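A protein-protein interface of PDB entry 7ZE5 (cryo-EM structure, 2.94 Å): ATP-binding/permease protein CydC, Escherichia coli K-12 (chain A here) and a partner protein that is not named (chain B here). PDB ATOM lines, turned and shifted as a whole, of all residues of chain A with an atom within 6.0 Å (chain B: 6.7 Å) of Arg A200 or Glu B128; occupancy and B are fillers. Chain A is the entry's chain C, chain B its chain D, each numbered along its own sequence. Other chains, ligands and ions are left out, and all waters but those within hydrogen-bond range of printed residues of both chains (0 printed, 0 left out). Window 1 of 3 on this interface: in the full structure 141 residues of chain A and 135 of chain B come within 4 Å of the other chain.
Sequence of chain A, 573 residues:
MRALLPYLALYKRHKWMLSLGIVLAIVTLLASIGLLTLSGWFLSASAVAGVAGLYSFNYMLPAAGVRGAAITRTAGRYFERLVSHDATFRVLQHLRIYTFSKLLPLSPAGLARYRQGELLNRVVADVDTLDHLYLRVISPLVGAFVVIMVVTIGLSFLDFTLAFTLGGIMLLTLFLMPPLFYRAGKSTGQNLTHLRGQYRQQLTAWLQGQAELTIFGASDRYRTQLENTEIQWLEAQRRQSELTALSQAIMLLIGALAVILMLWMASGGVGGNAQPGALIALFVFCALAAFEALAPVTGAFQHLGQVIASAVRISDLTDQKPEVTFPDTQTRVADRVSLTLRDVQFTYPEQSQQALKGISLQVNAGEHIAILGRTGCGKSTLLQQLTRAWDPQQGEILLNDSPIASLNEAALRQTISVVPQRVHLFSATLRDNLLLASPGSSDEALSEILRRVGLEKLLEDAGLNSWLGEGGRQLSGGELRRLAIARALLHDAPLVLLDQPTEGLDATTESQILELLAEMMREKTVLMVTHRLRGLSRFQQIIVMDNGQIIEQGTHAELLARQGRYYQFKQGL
The guanidinium group (NH1) of Arg A200 lies within salt-bridge range of the side-chain carboxylate (OE1) of Glu B128, 3.1 Å away.
O of Gln A201 is in hydrogen-bond range of OG1 of Thr A204, 3.0 Å away. The backbone carbonyl oxygen (O) of Leu B198 lies within hydrogen-bond range of the side-chain hydroxyl (OG) of Ser B202. OD1 of Asn A121 lies within hydrogen-bond range of NE of Arg A200, at 2.6 Å. The side-chain carboxylate (OE1) of Glu B128 lies within hydrogen-bond range of the side-chain hydroxyl (OG1) of Thr B124 (3.2 Å). The backbone carbonyl oxygen of Arg A200 is in hydrogen-bond range of the side-chain hydroxyl of Thr A204, 2.8 Å away. The side-chain carboxylate of Asp B131 lies within salt-bridge range of the guanidinium group of Arg B99 (3.5 Å).
Ser B202 touches Leu A120. Val A124 touches Ser B202. Leu B127 touches Arg A196 (CD2 to O, 3.9 Å). Tyr A199 touches Arg B99 (OH to CD, 3.2 Å). Tyr A199 touches Val B126. Tyr A199 touches Leu B127 (CD2 to CD1, 3.5 Å). CB of Ala B123 touches CG of Arg A200 (3.98 Å). CD2 of Leu A203 touches CB of Val B126, 3.9 Å away. Leu A203 touches Leu B127. Thr A204 touches Ala B123 (CG2 to CB, 3.95 Å).
Of the printed residues of chain B, Arg A200 touches Ala B123, Leu B127 and Glu B128. Glu B128 touches one residue of chain A. Of the printed residues of chain A, Leu B127 touches Arg A196 (3.9 Å), Tyr A199 (3.5 Å), Arg A200 (3.6 Å) and Leu A203 (3.6 Å). Of the printed residues of chain A, Val B126 touches Tyr A199 and Leu A203. Printed residues of chain B within 4 Å of Leu A203: Ala B123, Val B126 and Leu B127. Phe B195 touches none of the printed residues of chain A. Ala A125 touches none of the printed residues of chain B.
Printed residues of chain A that touch a printed residue of chain B: Leu A120, Val A124, Arg A196, Tyr A199, Arg A200, Leu A203 and Thr A204. Hydrophobic or aromatic side chains of chain A that line the printed part of chain B: Leu A120, Val A124, Tyr A199 and Leu A203. Of the 17 printed residues of chain B, 6 touch a printed residue of chain A. Printed residues of chain B that touch a printed residue of chain A: Arg B99, Ala B123, Val B126, Leu B127, Glu B128 and Ser B202. Among the printed residues, 13 pairs touch across the chains. Among the printed residues, Asp or Glu carboxylates within 4 Å of a Lys or Arg side-chain nitrogen of the other chain: Arg A200 with Glu B128 (2.3 Å).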
ATOM      1  N   GLY A 117      25.438 -24.848 -29.421  1.00  0.00           N
ATOM      2  CA  GLY A 117      25.303 -24.839 -27.976  1.00  0.00           C
ATOM      3  C   GLY A 117      26.444 -24.159 -27.255  1.00  0.00           C
ATOM      4  O   GLY A 117      26.241 -23.590 -26.178  1.00  0.00           O
ATOM      5  N   GLU A 118      27.652 -24.197 -27.823  1.00  0.00           N
ATOM      6  CA  GLU A 118      28.778 -23.523 -27.190  1.00  0.00           C
ATOM      7  C   GLU A 118      28.842 -22.052 -27.572  1.00  0.00           C
ATOM      8  O   GLU A 118      29.440 -21.254 -26.845  1.00  0.00           O
ATOM      9  CB  GLU A 118      30.097 -24.209 -27.549  1.00  0.00           C
ATOM     10  CG  GLU A 118      30.473 -24.123 -29.012  1.00  0.00           C
ATOM     11  CD  GLU A 118      31.749 -24.869 -29.336  1.00  0.00           C
ATOM     12  OE1 GLU A 118      32.332 -25.477 -28.415  1.00  0.00           O
ATOM     13  OE2 GLU A 118      32.170 -24.849 -30.511  1.00  0.00           O
ATOM     14  N   LEU A 120      26.137 -20.236 -27.624  1.00  0.00           N
ATOM     15  CA  LEU A 120      25.277 -19.691 -26.581  1.00  0.00           C
ATOM     16  C   LEU A 120      26.037 -19.547 -25.272  1.00  0.00           C
ATOM     17  O   LEU A 120      25.894 -18.542 -24.570  1.00  0.00           O
ATOM     18  CB  LEU A 120      24.047 -20.579 -26.400  1.00  0.00           C
ATOM     19  CG  LEU A 120      23.304 -20.495 -25.068  1.00  0.00           C
ATOM     20  CD1 LEU A 120      22.542 -19.188 -24.970  1.00  0.00           C
ATOM     21  CD2 LEU A 120      22.371 -21.679 -24.907  1.00  0.00           C
ATOM     22  N   ASN A 121      26.860 -20.539 -24.937  1.00  0.00           N
ATOM     23  CA  ASN A 121      27.640 -20.480 -23.706  1.00  0.00           C
ATOM     24  C   ASN A 121      28.615 -19.310 -23.720  1.00  0.00           C
ATOM     25  O   ASN A 121      28.890 -18.712 -22.675  1.00  0.00           O
ATOM     26  CB  ASN A 121      28.385 -21.797 -23.506  1.00  0.00           C
ATOM     27  CG  ASN A 121      28.855 -21.987 -22.086  1.00  0.00           C
ATOM     28  OD1 ASN A 121      28.053 -22.185 -21.177  1.00  0.00           O
ATOM     29  ND2 ASN A 121      30.164 -21.933 -21.887  1.00  0.00           N
ATOM     30  N   VAL A 124      26.341 -15.714 -23.158  1.00  0.00           N
ATOM     31  CA  VAL A 124      25.580 -15.503 -21.935  1.00  0.00           C
ATOM     32  C   VAL A 124      26.314 -16.032 -20.709  1.00  0.00           C
ATOM     33  O   VAL A 124      26.104 -15.538 -19.603  1.00  0.00           O
ATOM     34  CB  VAL A 124      24.171 -16.126 -22.046  1.00  0.00           C
ATOM     35  CG1 VAL A 124      23.457 -15.615 -23.291  1.00  0.00           C
ATOM     36  CG2 VAL A 124      24.240 -17.642 -22.025  1.00  0.00           C
ATOM     37  N   ALA A 125      27.175 -17.035 -20.873  1.00  0.00           N
ATOM     38  CA  ALA A 125      27.820 -17.639 -19.713  1.00  0.00           C
ATOM     39  C   ALA A 125      29.286 -17.254 -19.589  1.00  0.00           C
ATOM     40  O   ALA A 125      29.769 -17.024 -18.477  1.00  0.00           O
ATOM     41  CB  ALA A 125      27.683 -19.161 -19.768  1.00  0.00           C
ATOM     42  N   LEU A 195      34.341 -27.585 -20.006  1.00  0.00           N
ATOM     43  CA  LEU A 195      33.333 -28.598 -19.722  1.00  0.00           C
ATOM     44  C   LEU A 195      31.943 -28.004 -19.556  1.00  0.00           C
ATOM     45  O   LEU A 195      30.950 -28.703 -19.776  1.00  0.00           O
ATOM     46  CB  LEU A 195      33.715 -29.387 -18.471  1.00  0.00           C
ATOM     47  CG  LEU A 195      34.824 -30.414 -18.675  1.00  0.00           C
ATOM     48  CD1 LEU A 195      35.301 -30.954 -17.345  1.00  0.00           C
ATOM     49  CD2 LEU A 195      34.345 -31.534 -19.568  1.00  0.00           C
ATOM     50  N   ARG A 196      31.843 -26.735 -19.158  1.00  0.00           N
ATOM     51  CA  ARG A 196      30.528 -26.112 -19.060  1.00  0.00           C
ATOM     52  C   ARG A 196      29.926 -25.884 -20.438  1.00  0.00           C
ATOM     53  O   ARG A 196      28.718 -26.055 -20.629  1.00  0.00           O
ATOM     54  CB  ARG A 196      30.615 -24.795 -18.294  1.00  0.00           C
ATOM     55  CG  ARG A 196      29.269 -24.113 -18.129  1.00  0.00           C
ATOM     56  CD  ARG A 196      29.375 -22.853 -17.306  1.00  0.00           C
ATOM     57  NE  ARG A 196      30.468 -22.006 -17.765  1.00  0.00           N
ATOM     58  CZ  ARG A 196      30.618 -20.733 -17.422  1.00  0.00           C
ATOM     59  NH1 ARG A 196      29.742 -20.156 -16.615  1.00  0.00           N
ATOM     60  NH2 ARG A 196      31.647 -20.037 -17.888  1.00  0.00           N
ATOM     61  N   GLY A 197      30.751 -25.498 -21.411  1.00  0.00           N
ATOM     62  CA  GLY A 197      30.250 -25.319 -22.761  1.00  0.00           C
ATOM     63  C   GLY A 197      30.005 -26.630 -23.474  1.00  0.00           C
ATOM     64  O   GLY A 197      29.153 -26.705 -24.363  1.00  0.00           O
ATOM     65  N   GLN A 198      30.719 -27.674 -23.050  1.00  0.00           N
ATOM     66  CA  GLN A 198      30.524 -29.023 -23.638  1.00  0.00           C
ATOM     67  C   GLN A 198      29.199 -29.577 -23.111  1.00  0.00           C
ATOM     68  O   GLN A 198      28.470 -30.196 -23.897  1.00  0.00           O
ATOM     69  CB  GLN A 198      31.678 -29.953 -23.267  1.00  0.00           C
ATOM     70  CG  GLN A 198      31.713 -31.213 -24.117  1.00  0.00           C
ATOM     71  CD  GLN A 198      32.687 -32.245 -23.607  1.00  0.00           C
ATOM     72  OE1 GLN A 198      33.511 -32.769 -24.350  1.00  0.00           O
ATOM     73  NE2 GLN A 198      32.593 -32.551 -22.325  1.00  0.00           N
ATOM     74  N   TYR A 199      28.890 -29.327 -21.835  1.00  0.00           N
ATOM     75  CA  TYR A 199      27.641 -29.811 -21.260  1.00  0.00           C
ATOM     76  C   TYR A 199      26.446 -29.047 -21.812  1.00  0.00           C
ATOM     77  O   TYR A 199      25.402 -29.643 -22.095  1.00  0.00           O
ATOM     78  CB  TYR A 199      27.685 -29.710 -19.735  1.00  0.00           C
ATOM     79  CG  TYR A 199      26.476 -30.311 -19.060  1.00  0.00           C
ATOM     80  CD1 TYR A 199      26.452 -31.646 -18.707  1.00  0.00           C
ATOM     81  CD2 TYR A 199      25.359 -29.544 -18.778  1.00  0.00           C
ATOM     82  CE1 TYR A 199      25.353 -32.200 -18.097  1.00  0.00           C
ATOM     83  CE2 TYR A 199      24.255 -30.091 -18.169  1.00  0.00           C
ATOM     84  CZ  TYR A 199      24.257 -31.419 -17.832  1.00  0.00           C
ATOM     85  OH  TYR A 199      23.159 -31.973 -17.223  1.00  0.00           O
ATOM     86  N   ARG A 200      26.573 -27.729 -21.965  1.00  0.00           N
ATOM     87  CA  ARG A 200      25.465 -26.946 -22.501  1.00  0.00           C
ATOM     88  C   ARG A 200      25.200 -27.273 -23.963  1.00  0.00           C
ATOM     89  O   ARG A 200      24.050 -27.216 -24.408  1.00  0.00           O
ATOM     90  CB  ARG A 200      25.738 -25.455 -22.333  1.00  0.00           C
ATOM     91  CG  ARG A 200      24.575 -24.579 -22.736  1.00  0.00           C
ATOM     92  CD  ARG A 200      24.918 -23.119 -22.592  1.00  0.00           C
ATOM     93  NE  ARG A 200      25.577 -22.847 -21.323  1.00  0.00           N
ATOM     94  CZ  ARG A 200      24.995 -22.232 -20.302  1.00  0.00           C
ATOM     95  NH1 ARG A 200      23.740 -21.822 -20.402  1.00  0.00           N
ATOM     96  NH2 ARG A 200      25.669 -22.026 -19.181  1.00  0.00           N
ATOM     97  N   GLN A 201      26.241 -27.609 -24.725  1.00  0.00           N
ATOM     98  CA  GLN A 201      26.031 -28.043 -26.101  1.00  0.00           C
ATOM     99  C   GLN A 201      25.359 -29.407 -26.146  1.00  0.00           C
ATOM    100  O   GLN A 201      24.378 -29.601 -26.872  1.00  0.00           O
ATOM    101  CB  GLN A 201      27.360 -28.069 -26.854  1.00  0.00           C
ATOM    102  CG  GLN A 201      27.404 -29.023 -28.043  1.00  0.00           C
ATOM    103  CD  GLN A 201      26.301 -28.779 -29.061  1.00  0.00           C
ATOM    104  OE1 GLN A 201      25.896 -27.645 -29.299  1.00  0.00           O
ATOM    105  NE2 GLN A 201      25.824 -29.851 -29.677  1.00  0.00           N
ATOM    106  N   GLN A 202      25.867 -30.368 -25.373  1.00  0.00           N
ATOM    107  CA  GLN A 202      25.282 -31.702 -25.397  1.00  0.00           C
ATOM    108  C   GLN A 202      23.861 -31.702 -24.857  1.00  0.00           C
ATOM    109  O   GLN A 202      23.042 -32.523 -25.277  1.00  0.00           O
ATOM    110  CB  GLN A 202      26.148 -32.675 -24.604  1.00  0.00           C
ATOM    111  CG  GLN A 202      27.491 -32.965 -25.229  1.00  0.00           C
ATOM    112  CD  GLN A 202      28.331 -33.887 -24.380  1.00  0.00           C
ATOM    113  OE1 GLN A 202      28.156 -33.959 -23.168  1.00  0.00           O
ATOM    114  NE2 GLN A 202      29.252 -34.597 -25.011  1.00  0.00           N
ATOM    115  N   LEU A 203      23.549 -30.798 -23.928  1.00  0.00           N
ATOM    116  CA  LEU A 203      22.196 -30.736 -23.389  1.00  0.00           C
ATOM    117  C   LEU A 203      21.222 -30.145 -24.400  1.00  0.00           C
ATOM    118  O   LEU A 203      20.117 -30.666 -24.579  1.00  0.00           O
ATOM    119  CB  LEU A 203      22.184 -29.929 -22.095  1.00  0.00           C
ATOM    120  CG  LEU A 203      20.810 -29.567 -21.536  1.00  0.00           C
ATOM    121  CD1 LEU A 203      20.232 -30.730 -20.764  1.00  0.00           C
ATOM    122  CD2 LEU A 203      20.915 -28.343 -20.661  1.00  0.00           C
ATOM    123  N   THR A 204      21.610 -29.058 -25.071  1.00  0.00           N
ATOM    124  CA  THR A 204      20.729 -28.454 -26.065  1.00  0.00           C
ATOM    125  C   THR A 204      20.561 -29.360 -27.277  1.00  0.00           C
ATOM    126  O   THR A 204      19.466 -29.450 -27.843  1.00  0.00           O
ATOM    127  CB  THR A 204      21.261 -27.090 -26.494  1.00  0.00           C
ATOM    128  OG1 THR A 204      22.636 -27.210 -26.873  1.00  0.00           O
ATOM    129  CG2 THR A 204      21.134 -26.089 -25.362  1.00  0.00           C
ATOM    130  N   ALA A 205      21.635 -30.031 -27.696  1.00  0.00           N
ATOM    131  CA  ALA A 205      21.525 -30.985 -28.792  1.00  0.00           C
ATOM    132  C   ALA A 205      20.647 -32.165 -28.403  1.00  0.00           C
ATOM    133  O   ALA A 205      19.909 -32.704 -29.234  1.00  0.00           O
ATOM    134  CB  ALA A 205      22.912 -31.461 -29.212  1.00  0.00           C
ATOM    135  N   LEU A 226      25.850 -37.458 -21.748  1.00  0.00           N
ATOM    136  CA  LEU A 226      25.580 -36.113 -21.173  1.00  0.00           C
ATOM    137  C   LEU A 226      25.932 -36.116 -19.683  1.00  0.00           C
ATOM    138  O   LEU A 226      26.596 -35.168 -19.237  1.00  0.00           O
ATOM    139  CB  LEU A 226      24.103 -35.771 -21.384  1.00  0.00           C
ATOM    140  CG  LEU A 226      23.663 -34.425 -20.817  1.00  0.00           C
ATOM    141  CD1 LEU A 226      24.604 -33.321 -21.271  1.00  0.00           C
ATOM    142  CD2 LEU A 226      22.232 -34.107 -21.212  1.00  0.00           C
ATOM    143  N   ARG B  99      19.596 -32.324 -10.495  1.00  0.00           N
ATOM    144  CA  ARG B  99      19.716 -32.305 -11.949  1.00  0.00           C
ATOM    145  C   ARG B  99      19.300 -33.634 -12.559  1.00  0.00           C
ATOM    146  O   ARG B  99      18.729 -33.668 -13.652  1.00  0.00           O
ATOM    147  CB  ARG B  99      21.141 -31.952 -12.359  1.00  0.00           C
ATOM    148  CG  ARG B  99      21.295 -31.699 -13.842  1.00  0.00           C
ATOM    149  CD  ARG B  99      22.692 -31.236 -14.171  1.00  0.00           C
ATOM    150  NE  ARG B  99      22.909 -29.850 -13.780  1.00  0.00           N
ATOM    151  CZ  ARG B  99      23.888 -29.447 -12.982  1.00  0.00           C
ATOM    152  NH1 ARG B  99      24.744 -30.327 -12.485  1.00  0.00           N
ATOM    153  NH2 ARG B  99      24.009 -28.166 -12.679  1.00  0.00           N
ATOM    154  N   GLY B 120      17.219 -22.529 -25.199  1.00  0.00           N
ATOM    155  CA  GLY B 120      18.108 -21.772 -24.342  1.00  0.00           C
ATOM    156  C   GLY B 120      17.562 -21.518 -22.957  1.00  0.00           C
ATOM    157  O   GLY B 120      18.340 -21.258 -22.035  1.00  0.00           O
ATOM    158  N   ALA B 123      18.442 -24.742 -20.997  1.00  0.00           N
ATOM    159  CA  ALA B 123      19.857 -24.819 -20.653  1.00  0.00           C
ATOM    160  C   ALA B 123      20.173 -24.000 -19.409  1.00  0.00           C
ATOM    161  O   ALA B 123      20.927 -24.446 -18.538  1.00  0.00           O
ATOM    162  CB  ALA B 123      20.706 -24.356 -21.834  1.00  0.00           C
ATOM    163  N   THR B 124      19.609 -22.800 -19.306  1.00  0.00           N
ATOM    164  CA  THR B 124      19.826 -21.973 -18.129  1.00  0.00           C
ATOM    165  C   THR B 124      19.004 -22.423 -16.931  1.00  0.00           C
ATOM    166  O   THR B 124      19.214 -21.910 -15.829  1.00  0.00           O
ATOM    167  CB  THR B 124      19.511 -20.512 -18.441  1.00  0.00           C
ATOM    168  OG1 THR B 124      19.678 -19.727 -17.256  1.00  0.00           O
ATOM    169  CG2 THR B 124      18.097 -20.376 -18.921  1.00  0.00           C
ATOM    170  N   LEU B 125      18.077 -23.357 -17.120  1.00  0.00           N
ATOM    171  CA  LEU B 125      17.343 -23.951 -16.015  1.00  0.00           C
ATOM    172  C   LEU B 125      18.037 -25.191 -15.477  1.00  0.00           C
ATOM    173  O   LEU B 125      17.852 -25.541 -14.308  1.00  0.00           O
ATOM    174  CB  LEU B 125      15.923 -24.301 -16.464  1.00  0.00           C
ATOM    175  CG  LEU B 125      14.880 -24.773 -15.453  1.00  0.00           C
ATOM    176  CD1 LEU B 125      13.528 -24.231 -15.856  1.00  0.00           C
ATOM    177  CD2 LEU B 125      14.827 -26.287 -15.371  1.00  0.00           C
ATOM    178  N   VAL B 126      18.833 -25.855 -16.307  1.00  0.00           N
ATOM    179  CA  VAL B 126      19.558 -27.042 -15.878  1.00  0.00           C
ATOM    180  C   VAL B 126      20.964 -26.698 -15.398  1.00  0.00           C
ATOM    181  O   VAL B 126      21.475 -27.337 -14.474  1.00  0.00           O
ATOM    182  CB  VAL B 126      19.591 -28.072 -17.019  1.00  0.00           C
ATOM    183  CG1 VAL B 126      20.475 -29.250 -16.665  1.00  0.00           C
ATOM    184  CG2 VAL B 126      18.187 -28.541 -17.342  1.00  0.00           C
ATOM    185  N   LEU B 127      21.604 -25.691 -15.991  1.00  0.00           N
ATOM    186  CA  LEU B 127      22.950 -25.318 -15.569  1.00  0.00           C
ATOM    187  C   LEU B 127      22.937 -24.187 -14.544  1.00  0.00           C
ATOM    188  O   LEU B 127      23.377 -24.372 -13.407  1.00  0.00           O
ATOM    189  CB  LEU B 127      23.801 -24.921 -16.780  1.00  0.00           C
ATOM    190  CG  LEU B 127      24.403 -26.030 -17.645  1.00  0.00           C
ATOM    191  CD1 LEU B 127      23.362 -26.661 -18.550  1.00  0.00           C
ATOM    192  CD2 LEU B 127      25.569 -25.500 -18.452  1.00  0.00           C
ATOM    193  N   GLU B 128      22.423 -23.017 -14.924  1.00  0.00           N
ATOM    194  CA  GLU B 128      22.538 -21.850 -14.054  1.00  0.00           C
ATOM    195  C   GLU B 128      21.615 -21.946 -12.846  1.00  0.00           C
ATOM    196  O   GLU B 128      22.030 -21.667 -11.717  1.00  0.00           O
ATOM    197  CB  GLU B 128      22.264 -20.572 -14.843  1.00  0.00           C
ATOM    198  CG  GLU B 128      23.469 -20.059 -15.608  1.00  0.00           C
ATOM    199  CD  GLU B 128      23.633 -20.704 -16.963  1.00  0.00           C
ATOM    200  OE1 GLU B 128      22.732 -20.551 -17.811  1.00  0.00           O
ATOM    201  OE2 GLU B 128      24.673 -21.358 -17.185  1.00  0.00           O
ATOM    202  N   GLN B 129      20.360 -22.335 -13.060  1.00  0.00           N
ATOM    203  CA  GLN B 129      19.404 -22.318 -11.958  1.00  0.00           C
ATOM    204  C   GLN B 129      19.710 -23.405 -10.932  1.00  0.00           C
ATOM    205  O   GLN B 129      19.596 -23.170  -9.725  1.00  0.00           O
ATOM    206  CB  GLN B 129      17.982 -22.456 -12.495  1.00  0.00           C
ATOM    207  CG  GLN B 129      17.324 -21.127 -12.791  1.00  0.00           C
ATOM    208  CD  GLN B 129      15.897 -21.272 -13.259  1.00  0.00           C
ATOM    209  OE1 GLN B 129      15.103 -21.984 -12.651  1.00  0.00           O
ATOM    210  NE2 GLN B 129      15.559 -20.588 -14.343  1.00  0.00           N
ATOM    211  N   ILE B 130      20.097 -24.595 -11.389  1.00  0.00           N
ATOM    212  CA  ILE B 130      20.405 -25.677 -10.459  1.00  0.00           C
ATOM    213  C   ILE B 130      21.708 -25.397  -9.716  1.00  0.00           C
ATOM    214  O   ILE B 130      21.820 -25.666  -8.516  1.00  0.00           O
ATOM    215  CB  ILE B 130      20.448 -27.023 -11.201  1.00  0.00           C
ATOM    216  CG1 ILE B 130      19.046 -27.412 -11.662  1.00  0.00           C
ATOM    217  CG2 ILE B 130      21.015 -28.110 -10.310  1.00  0.00           C
ATOM    218  CD1 ILE B 130      18.988 -28.716 -12.408  1.00  0.00           C
ATOM    219  N   ASP B 131      22.709 -24.850 -10.409  1.00  0.00           N
ATOM    220  CA  ASP B 131      23.997 -24.603  -9.770  1.00  0.00           C
ATOM    221  C   ASP B 131      23.949 -23.451  -8.780  1.00  0.00           C
ATOM    222  O   ASP B 131      24.848 -23.337  -7.944  1.00  0.00           O
ATOM    223  CB  ASP B 131      25.073 -24.325 -10.818  1.00  0.00           C
ATOM    224  CG  ASP B 131      25.453 -25.559 -11.603  1.00  0.00           C
ATOM    225  OD1 ASP B 131      24.991 -26.659 -11.244  1.00  0.00           O
ATOM    226  OD2 ASP B 131      26.216 -25.429 -12.580  1.00  0.00           O
ATOM    227  N   ASP B 132      22.936 -22.597  -8.852  1.00  0.00           N
ATOM    228  CA  ASP B 132      22.792 -21.505  -7.902  1.00  0.00           C
ATOM    229  C   ASP B 132      22.045 -21.911  -6.643  1.00  0.00           C
ATOM    230  O   ASP B 132      21.796 -21.058  -5.787  1.00  0.00           O
ATOM    231  CB  ASP B 132      22.095 -20.313  -8.560  1.00  0.00           C
ATOM    232  CG  ASP B 132      22.960 -19.645  -9.608  1.00  0.00           C
ATOM    233  OD1 ASP B 132      24.199 -19.690  -9.477  1.00  0.00           O
ATOM    234  OD2 ASP B 132      22.407 -19.062 -10.558  1.00  0.00           O
ATOM    235  N   MET B 133      21.674 -23.179  -6.513  1.00  0.00           N
ATOM    236  CA  MET B 133      21.183 -23.713  -5.254  1.00  0.00           C
ATOM    237  C   MET B 133      22.301 -24.250  -4.375  1.00  0.00           C
ATOM    238  O   MET B 133      22.028 -24.707  -3.263  1.00  0.00           O
ATOM    239  CB  MET B 133      20.159 -24.824  -5.504  1.00  0.00           C
ATOM    240  CG  MET B 133      19.023 -24.440  -6.424  1.00  0.00           C
ATOM    241  SD  MET B 133      17.954 -25.839  -6.789  1.00  0.00           S
ATOM    242  CE  MET B 133      16.863 -25.115  -8.002  1.00  0.00           C
ATOM    243  N   PHE B 195      16.274 -14.798 -12.772  1.00  0.00           N
ATOM    244  CA  PHE B 195      16.404 -15.975 -13.619  1.00  0.00           C
ATOM    245  C   PHE B 195      15.395 -15.952 -14.754  1.00  0.00           C
ATOM    246  O   PHE B 195      15.619 -16.573 -15.796  1.00  0.00           O
ATOM    247  CB  PHE B 195      16.237 -17.241 -12.785  1.00  0.00           C
ATOM    248  CG  PHE B 195      17.384 -17.507 -11.865  1.00  0.00           C
ATOM    249  CD1 PHE B 195      18.632 -17.805 -12.371  1.00  0.00           C
ATOM    250  CD2 PHE B 195      17.217 -17.451 -10.496  1.00  0.00           C
ATOM    251  CE1 PHE B 195      19.689 -18.049 -11.531  1.00  0.00           C
ATOM    252  CE2 PHE B 195      18.274 -17.692  -9.651  1.00  0.00           C
ATOM    253  CZ  PHE B 195      19.510 -17.993 -10.169  1.00  0.00           C
ATOM    254  N   LEU B 198      17.235 -13.962 -17.279  1.00  0.00           N
ATOM    255  CA  LEU B 198      18.326 -14.745 -17.847  1.00  0.00           C
ATOM    256  C   LEU B 198      17.798 -15.818 -18.786  1.00  0.00           C
ATOM    257  O   LEU B 198      18.403 -16.094 -19.827  1.00  0.00           O
ATOM    258  CB  LEU B 198      19.158 -15.375 -16.733  1.00  0.00           C
ATOM    259  CG  LEU B 198      20.237 -16.362 -17.172  1.00  0.00           C
ATOM    260  CD1 LEU B 198      21.195 -15.708 -18.145  1.00  0.00           C
ATOM    261  CD2 LEU B 198      20.979 -16.906 -15.973  1.00  0.00           C
ATOM    262  N   SER B 202      18.863 -15.994 -22.624  1.00  0.00           N
ATOM    263  CA  SER B 202      19.448 -17.232 -23.127  1.00  0.00           C
ATOM    264  C   SER B 202      18.570 -17.869 -24.194  1.00  0.00           C
ATOM    265  O   SER B 202      19.075 -18.365 -25.206  1.00  0.00           O
ATOM    266  CB  SER B 202      19.679 -18.213 -21.982  1.00  0.00           C
ATOM    267  OG  SER B 202      20.709 -17.765 -21.124  1.00  0.00           O
ATOM    268  N   ALA B 320      15.519 -19.641  -7.811  1.00  0.00           N
ATOM    269  CA  ALA B 320      15.919 -20.623  -8.811  1.00  0.00           C
ATOM    270  C   ALA B 320      14.993 -21.831  -8.821  1.00  0.00           C
ATOM    271  O   ALA B 320      14.833 -22.477  -9.860  1.00  0.00           O
ATOM    272  CB  ALA B 320      17.360 -21.063  -8.566  1.00  0.00           C
